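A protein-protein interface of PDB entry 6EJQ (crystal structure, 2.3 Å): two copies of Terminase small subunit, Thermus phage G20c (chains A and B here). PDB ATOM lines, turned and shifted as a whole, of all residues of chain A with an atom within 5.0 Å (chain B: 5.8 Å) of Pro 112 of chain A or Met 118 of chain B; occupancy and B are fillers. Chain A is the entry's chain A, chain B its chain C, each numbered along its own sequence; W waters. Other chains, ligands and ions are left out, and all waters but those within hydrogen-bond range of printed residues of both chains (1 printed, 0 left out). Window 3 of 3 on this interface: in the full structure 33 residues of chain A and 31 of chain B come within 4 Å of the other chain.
Among the printed residues, merely in contact across the chains: Pro 112 of chain A with Met 118 of chain B, Pro 112 of chain A with Met 87 of chain B, Pro 112 of chain A with Ile 83 of chain B, Tyr 91 of chain A with Ile 83 of chain B, Ala 116 of chain A with Arg 121 of chain B, Ile 115 of chain A with Ile 83 of chain B and Ala 116 of chain A with Leu 80 of chain B.
Of the printed residues of chain B, Tyr 91 of chain A touches Ile 83. Of the printed residues of chain B, Ile 115 of chain A touches Ile 83 (3.9 Å). Of the printed residues of chain A, Ile 83 of chain B touches Tyr 91 (3.8 Å), Pro 112 (3.7 Å) and Ile 115 (3.9 Å). Of the printed residues of chain A, Met 87 of chain B touches Pro 112. Of the printed residues of chain A, Met 118 of chain B touches Pro 112 (3.4 Å). Of the printed residues of chain A, Arg 121 of chain B touches Ala 116. The nearest residue of chain B that does not touch Pro 112 of chain A is Leu 80 of chain B (5.1 Å).
Printed residues of chain A that touch a printed residue of chain B: Tyr 91, Pro 112, Ile 115 and Ala 116. Along chain A the printed residues that touch a printed residue of chain B span positions 91 to 116. Printed residues of chain B that touch a printed residue of chain A: Leu 80, Ile 83, Met 87, Met 118 and Arg 121. Hydrophobic or aromatic side chains of chain B that line the printed part of chain A: Leu 80, Ile 83, Met 87 and Met 118. Among the printed residues, 7 pairs touch across the chains.
4 positions are printed for both chains. Of the 7 pairs that touch across the chains among the printed residues, none has its exchanged pair printed and touching as well.
Water W1 lies within hydrogen-bond range of NH2 of Arg 121 of chain B and O of Ala 113 of chain A.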
ATOM      1  N   TYR A  91      20.872  -3.377  -3.852  1.00  0.00           N
ATOM      2  CA  TYR A  91      19.839  -3.117  -2.859  1.00  0.00           C
ATOM      3  C   TYR A  91      19.044  -1.860  -3.180  1.00  0.00           C
ATOM      4  O   TYR A  91      17.821  -1.861  -3.078  1.00  0.00           O
ATOM      5  CB  TYR A  91      20.442  -3.003  -1.449  1.00  0.00           C
ATOM      6  CG  TYR A  91      19.401  -2.715  -0.391  1.00  0.00           C
ATOM      7  CD1 TYR A  91      18.546  -3.716   0.039  1.00  0.00           C
ATOM      8  CD2 TYR A  91      19.252  -1.437   0.155  1.00  0.00           C
ATOM      9  CE1 TYR A  91      17.572  -3.466   0.991  1.00  0.00           C
ATOM     10  CE2 TYR A  91      18.273  -1.173   1.108  1.00  0.00           C
ATOM     11  CZ  TYR A  91      17.442  -2.199   1.523  1.00  0.00           C
ATOM     12  OH  TYR A  91      16.467  -1.987   2.459  1.00  0.00           O
ATOM     13  N   VAL A 110      19.376  -8.811  -3.091  1.00  0.00           N
ATOM     14  CA  VAL A 110      20.295  -8.701  -1.962  1.00  0.00           C
ATOM     15  C   VAL A 110      19.471  -8.346  -0.739  1.00  0.00           C
ATOM     16  O   VAL A 110      18.713  -7.388  -0.768  1.00  0.00           O
ATOM     17  CB  VAL A 110      21.338  -7.573  -2.175  1.00  0.00           C
ATOM     18  CG1 VAL A 110      22.244  -7.431  -0.957  1.00  0.00           C
ATOM     19  CG2 VAL A 110      22.193  -7.840  -3.397  1.00  0.00           C
ATOM     20  N   ARG A 111      19.643  -9.099   0.339  1.00  0.00           N
ATOM     21  CA  ARG A 111      18.914  -8.848   1.590  1.00  0.00           C
ATOM     22  C   ARG A 111      19.734  -7.956   2.530  1.00  0.00           C
ATOM     23  O   ARG A 111      20.967  -7.987   2.482  1.00  0.00           O
ATOM     24  CB  ARG A 111      18.581 -10.172   2.278  1.00  0.00           C
ATOM     25  CG  ARG A 111      17.683 -11.078   1.454  1.00  0.00           C
ATOM     26  CD  ARG A 111      17.442 -12.416   2.140  1.00  0.00           C
ATOM     27  NE  ARG A 111      18.597 -13.320   2.007  1.00  0.00           N
ATOM     28  CZ  ARG A 111      19.377 -13.776   3.000  1.00  0.00           C
ATOM     29  NH1 ARG A 111      19.160 -13.454   4.284  1.00  0.00           N
ATOM     30  NH2 ARG A 111      20.395 -14.591   2.706  1.00  0.00           N
ATOM     31  N   PRO A 112      19.061  -7.153   3.389  1.00  0.00           N
ATOM     32  CA  PRO A 112      19.785  -6.362   4.387  1.00  0.00           C
ATOM     33  C   PRO A 112      20.782  -7.170   5.235  1.00  0.00           C
ATOM     34  O   PRO A 112      21.898  -6.693   5.490  1.00  0.00           O
ATOM     35  CB  PRO A 112      18.659  -5.795   5.252  1.00  0.00           C
ATOM     36  CG  PRO A 112      17.521  -5.636   4.309  1.00  0.00           C
ATOM     37  CD  PRO A 112      17.625  -6.810   3.374  1.00  0.00           C
ATOM     38  N   ALA A 113      20.376  -8.375   5.642  1.00  0.00           N
ATOM     39  CA  ALA A 113      21.238  -9.315   6.370  1.00  0.00           C
ATOM     40  C   ALA A 113      22.544  -9.672   5.634  1.00  0.00           C
ATOM     41  O   ALA A 113      23.586  -9.806   6.271  1.00  0.00           O
ATOM     42  CB  ALA A 113      20.468 -10.591   6.707  1.00  0.00           C
ATOM     43  N   ASP A 114      22.473  -9.842   4.313  1.00  0.00           N
ATOM     44  CA  ASP A 114      23.658 -10.092   3.476  1.00  0.00           C
ATOM     45  C   ASP A 114      24.650  -8.922   3.510  1.00  0.00           C
ATOM     46  O   ASP A 114      25.873  -9.142   3.541  1.00  0.00           O
ATOM     47  CB  ASP A 114      23.274 -10.318   2.001  1.00  0.00           C
ATOM     48  CG  ASP A 114      22.369 -11.539   1.777  1.00  0.00           C
ATOM     49  OD1 ASP A 114      22.415 -12.508   2.570  1.00  0.00           O
ATOM     50  OD2 ASP A 114      21.616 -11.512   0.768  1.00  0.00           O
ATOM     51  N   ILE A 115      24.120  -7.698   3.471  1.00  0.00           N
ATOM     52  CA  ILE A 115      24.930  -6.480   3.463  1.00  0.00           C
ATOM     53  C   ILE A 115      25.636  -6.324   4.810  1.00  0.00           C
ATOM     54  O   ILE A 115      26.844  -6.046   4.857  1.00  0.00           O
ATOM     55  CB  ILE A 115      24.077  -5.221   3.120  1.00  0.00           C
ATOM     56  CG1 ILE A 115      23.654  -5.271   1.647  1.00  0.00           C
ATOM     57  CG2 ILE A 115      24.842  -3.926   3.405  1.00  0.00           C
ATOM     58  CD1 ILE A 115      22.563  -4.295   1.234  1.00  0.00           C
ATOM     59  N   ALA A 116      24.877  -6.495   5.891  1.00  0.00           N
ATOM     60  CA  ALA A 116      25.433  -6.453   7.259  1.00  0.00           C
ATOM     61  C   ALA A 116      26.517  -7.516   7.461  1.00  0.00           C
ATOM     62  O   ALA A 116      27.596  -7.230   8.010  1.00  0.00           O
ATOM     63  CB  ALA A 116      24.331  -6.632   8.284  1.00  0.00           C
ATOM     64  N   LEU B  80      24.055   1.035   7.257  1.00  0.00           N
ATOM     65  CA  LEU B  80      23.103   0.136   7.893  1.00  0.00           C
ATOM     66  C   LEU B  80      21.929   0.873   8.527  1.00  0.00           C
ATOM     67  O   LEU B  80      20.811   0.363   8.520  1.00  0.00           O
ATOM     68  CB  LEU B  80      23.798  -0.751   8.935  1.00  0.00           C
ATOM     69  CG  LEU B  80      24.865  -1.729   8.431  1.00  0.00           C
ATOM     70  CD1 LEU B  80      25.342  -2.565   9.609  1.00  0.00           C
ATOM     71  CD2 LEU B  80      24.375  -2.633   7.306  1.00  0.00           C
ATOM     72  N   ILE B  83      19.540   1.640   5.675  1.00  0.00           N
ATOM     73  CA  ILE B  83      18.845   0.389   5.373  1.00  0.00           C
ATOM     74  C   ILE B  83      17.777   0.090   6.431  1.00  0.00           C
ATOM     75  O   ILE B  83      16.652  -0.293   6.086  1.00  0.00           O
ATOM     76  CB  ILE B  83      19.830  -0.793   5.222  1.00  0.00           C
ATOM     77  CG1 ILE B  83      20.671  -0.596   3.947  1.00  0.00           C
ATOM     78  CG2 ILE B  83      19.084  -2.124   5.148  1.00  0.00           C
ATOM     79  CD1 ILE B  83      21.940  -1.421   3.890  1.00  0.00           C
ATOM     80  N   TYR B  84      18.120   0.284   7.703  1.00  0.00           N
ATOM     81  CA  TYR B  84      17.170   0.048   8.792  1.00  0.00           C
ATOM     82  C   TYR B  84      15.895   0.882   8.616  1.00  0.00           C
ATOM     83  O   TYR B  84      14.797   0.368   8.832  1.00  0.00           O
ATOM     84  CB  TYR B  84      17.822   0.302  10.159  1.00  0.00           C
ATOM     85  CG  TYR B  84      16.888   0.177  11.341  1.00  0.00           C
ATOM     86  CD1 TYR B  84      16.689  -1.057  11.975  1.00  0.00           C
ATOM     87  CD2 TYR B  84      16.218   1.293  11.842  1.00  0.00           C
ATOM     88  CE1 TYR B  84      15.840  -1.175  13.059  1.00  0.00           C
ATOM     89  CE2 TYR B  84      15.370   1.188  12.924  1.00  0.00           C
ATOM     90  CZ  TYR B  84      15.180  -0.045  13.529  1.00  0.00           C
ATOM     91  OH  TYR B  84      14.335  -0.142  14.606  1.00  0.00           O
ATOM     92  N   MET B  87      13.752  -0.583   5.898  1.00  0.00           N
ATOM     93  CA  MET B  87      13.098  -1.801   6.416  1.00  0.00           C
ATOM     94  C   MET B  87      11.842  -1.476   7.218  1.00  0.00           C
ATOM     95  O   MET B  87      10.799  -2.083   6.998  1.00  0.00           O
ATOM     96  CB  MET B  87      14.067  -2.622   7.273  1.00  0.00           C
ATOM     97  CG  MET B  87      15.190  -3.264   6.475  1.00  0.00           C
ATOM     98  SD  MET B  87      16.516  -3.913   7.498  1.00  0.00           S
ATOM     99  CE  MET B  87      15.760  -5.426   8.068  1.00  0.00           C
ATOM    100  N   ALA B 113      12.000 -10.265  12.666  1.00  0.00           N
ATOM    101  CA  ALA B 113      13.322 -10.800  13.033  1.00  0.00           C
ATOM    102  C   ALA B 113      14.467 -10.128  12.263  1.00  0.00           C
ATOM    103  O   ALA B 113      15.559  -9.973  12.807  1.00  0.00           O
ATOM    104  CB  ALA B 113      13.372 -12.312  12.824  1.00  0.00           C
ATOM    105  N   ASP B 114      14.211  -9.733  11.013  1.00  0.00           N
ATOM    106  CA  ASP B 114      15.217  -9.057  10.185  1.00  0.00           C
ATOM    107  C   ASP B 114      15.490  -7.664  10.724  1.00  0.00           C
ATOM    108  O   ASP B 114      16.639  -7.252  10.815  1.00  0.00           O
ATOM    109  CB  ASP B 114      14.774  -8.931   8.718  1.00  0.00           C
ATOM    110  CG  ASP B 114      14.459 -10.273   8.056  1.00  0.00           C
ATOM    111  OD1 ASP B 114      14.987 -11.321   8.490  1.00  0.00           O
ATOM    112  OD2 ASP B 114      13.668 -10.249   7.082  1.00  0.00           O
ATOM    113  N   ILE B 115      14.424  -6.950  11.080  1.00  0.00           N
ATOM    114  CA  ILE B 115      14.536  -5.624  11.693  1.00  0.00           C
ATOM    115  C   ILE B 115      15.329  -5.679  13.002  1.00  0.00           C
ATOM    116  O   ILE B 115      16.244  -4.875  13.211  1.00  0.00           O
ATOM    117  CB  ILE B 115      13.149  -4.983  11.904  1.00  0.00           C
ATOM    118  CG1 ILE B 115      12.539  -4.625  10.539  1.00  0.00           C
ATOM    119  CG2 ILE B 115      13.234  -3.724  12.762  1.00  0.00           C
ATOM    120  CD1 ILE B 115      11.046  -4.396  10.557  1.00  0.00           C
ATOM    121  N   ALA B 116      14.997  -6.634  13.867  1.00  0.00           N
ATOM    122  CA  ALA B 116      15.722  -6.797  15.137  1.00  0.00           C
ATOM    123  C   ALA B 116      17.192  -7.158  14.917  1.00  0.00           C
ATOM    124  O   ALA B 116      18.080  -6.612  15.580  1.00  0.00           O
ATOM    125  CB  ALA B 116      15.040  -7.839  16.015  1.00  0.00           C
ATOM    126  N   ALA B 117      17.442  -8.059  13.974  1.00  0.00           N
ATOM    127  CA  ALA B 117      18.809  -8.453  13.629  1.00  0.00           C
ATOM    128  C   ALA B 117      19.632  -7.265  13.114  1.00  0.00           C
ATOM    129  O   ALA B 117      20.797  -7.110  13.491  1.00  0.00           O
ATOM    130  CB  ALA B 117      18.801  -9.584  12.601  1.00  0.00           C
ATOM    131  N   MET B 118      19.025  -6.417  12.283  1.00  0.00           N
ATOM    132  CA  MET B 118      19.708  -5.203  11.801  1.00  0.00           C
ATOM    133  C   MET B 118      19.954  -4.210  12.933  1.00  0.00           C
ATOM    134  O   MET B 118      21.033  -3.637  13.012  1.00  0.00           O
ATOM    135  CB  MET B 118      18.918  -4.521  10.674  1.00  0.00           C
ATOM    136  CG  MET B 118      19.620  -3.317  10.051  1.00  0.00           C
ATOM    137  SD  MET B 118      21.216  -3.738   9.338  1.00  0.00           S
ATOM    138  CE  MET B 118      20.646  -4.599   7.871  1.00  0.00           C
ATOM    139  N   ALA B 119      18.963  -4.008  13.802  1.00  0.00           N
ATOM    140  CA  ALA B 119      19.164  -3.158  14.987  1.00  0.00           C
ATOM    141  C   ALA B 119      20.346  -3.658  15.809  1.00  0.00           C
ATOM    142  O   ALA B 119      21.196  -2.873  16.201  1.00  0.00           O
ATOM    143  CB  ALA B 119      17.908  -3.103  15.846  1.00  0.00           C
ATOM    144  N   ASP B 120      20.405  -4.971  16.033  1.00  0.00           N
ATOM    145  CA  ASP B 120      21.502  -5.594  16.782  1.00  0.00           C
ATOM    146  C   ASP B 120      22.862  -5.408  16.095  1.00  0.00           C
ATOM    147  O   ASP B 120      23.856  -5.171  16.768  1.00  0.00           O
ATOM    148  CB  ASP B 120      21.231  -7.086  17.008  1.00  0.00           C
ATOM    149  CG  ASP B 120      22.322  -7.756  17.827  1.00  0.00           C
ATOM    150  OD1 ASP B 120      22.672  -7.222  18.904  1.00  0.00           O
ATOM    151  OD2 ASP B 120      22.840  -8.807  17.400  1.00  0.00           O
ATOM    152  N   ARG B 121      22.904  -5.512  14.768  1.00  0.00           N
ATOM    153  CA  ARG B 121      24.142  -5.227  14.016  1.00  0.00           C
ATOM    154  C   ARG B 121      24.620  -3.794  14.268  1.00  0.00           C
ATOM    155  O   ARG B 121      25.804  -3.557  14.485  1.00  0.00           O
ATOM    156  CB  ARG B 121      23.947  -5.424  12.507  1.00  0.00           C
ATOM    157  CG  ARG B 121      23.729  -6.864  12.063  1.00  0.00           C
ATOM    158  CD  ARG B 121      24.998  -7.696  12.153  1.00  0.00           C
ATOM    159  NE  ARG B 121      24.942  -8.884  11.302  1.00  0.00           N
ATOM    160  CZ  ARG B 121      25.952  -9.738  11.109  1.00  0.00           C
ATOM    161  NH1 ARG B 121      27.137  -9.566  11.697  1.00  0.00           N
ATOM    162  NH2 ARG B 121      25.778 -10.779  10.306  1.00  0.00           N
ATOM    163  N   ILE B 122      23.689  -2.849  14.260  1.00  0.00           N
ATOM    164  CA  ILE B 122      24.038  -1.448  14.450  1.00  0.00           C
ATOM    165  C   ILE B 122      24.523  -1.201  15.885  1.00  0.00           C
ATOM    166  O   ILE B 122      25.511  -0.501  16.091  1.00  0.00           O
ATOM    167  CB  ILE B 122      22.870  -0.529  14.080  1.00  0.00           C
ATOM    168  CG1 ILE B 122      22.567  -0.643  12.582  1.00  0.00           C
ATOM    169  CG2 ILE B 122      23.190   0.918  14.436  1.00  0.00           C
ATOM    170  CD1 ILE B 122      21.162  -0.224  12.183  1.00  0.00           C
ATOM    171  N   MET B 123      23.832  -1.789  16.861  1.00  0.00           N
ATOM    172  CA  MET B 123      24.211  -1.675  18.265  1.00  0.00           C
ATOM    173  C   MET B 123      25.537  -2.359  18.567  1.00  0.00           C
ATOM    174  O   MET B 123      26.302  -1.854  19.388  1.00  0.00           O
ATOM    175  CB  MET B 123      23.109  -2.228  19.177  1.00  0.00           C
ATOM    176  CG  MET B 123      21.861  -1.358  19.187  1.00  0.00           C
ATOM    177  SD  MET B 123      20.593  -1.920  20.331  1.00  0.00           S
ATOM    178  CE  MET B 123      20.137  -3.511  19.658  1.00  0.00           C
HETATM  179  O   HOH W   1      23.216 -10.383   9.130  1.00  0.00           O
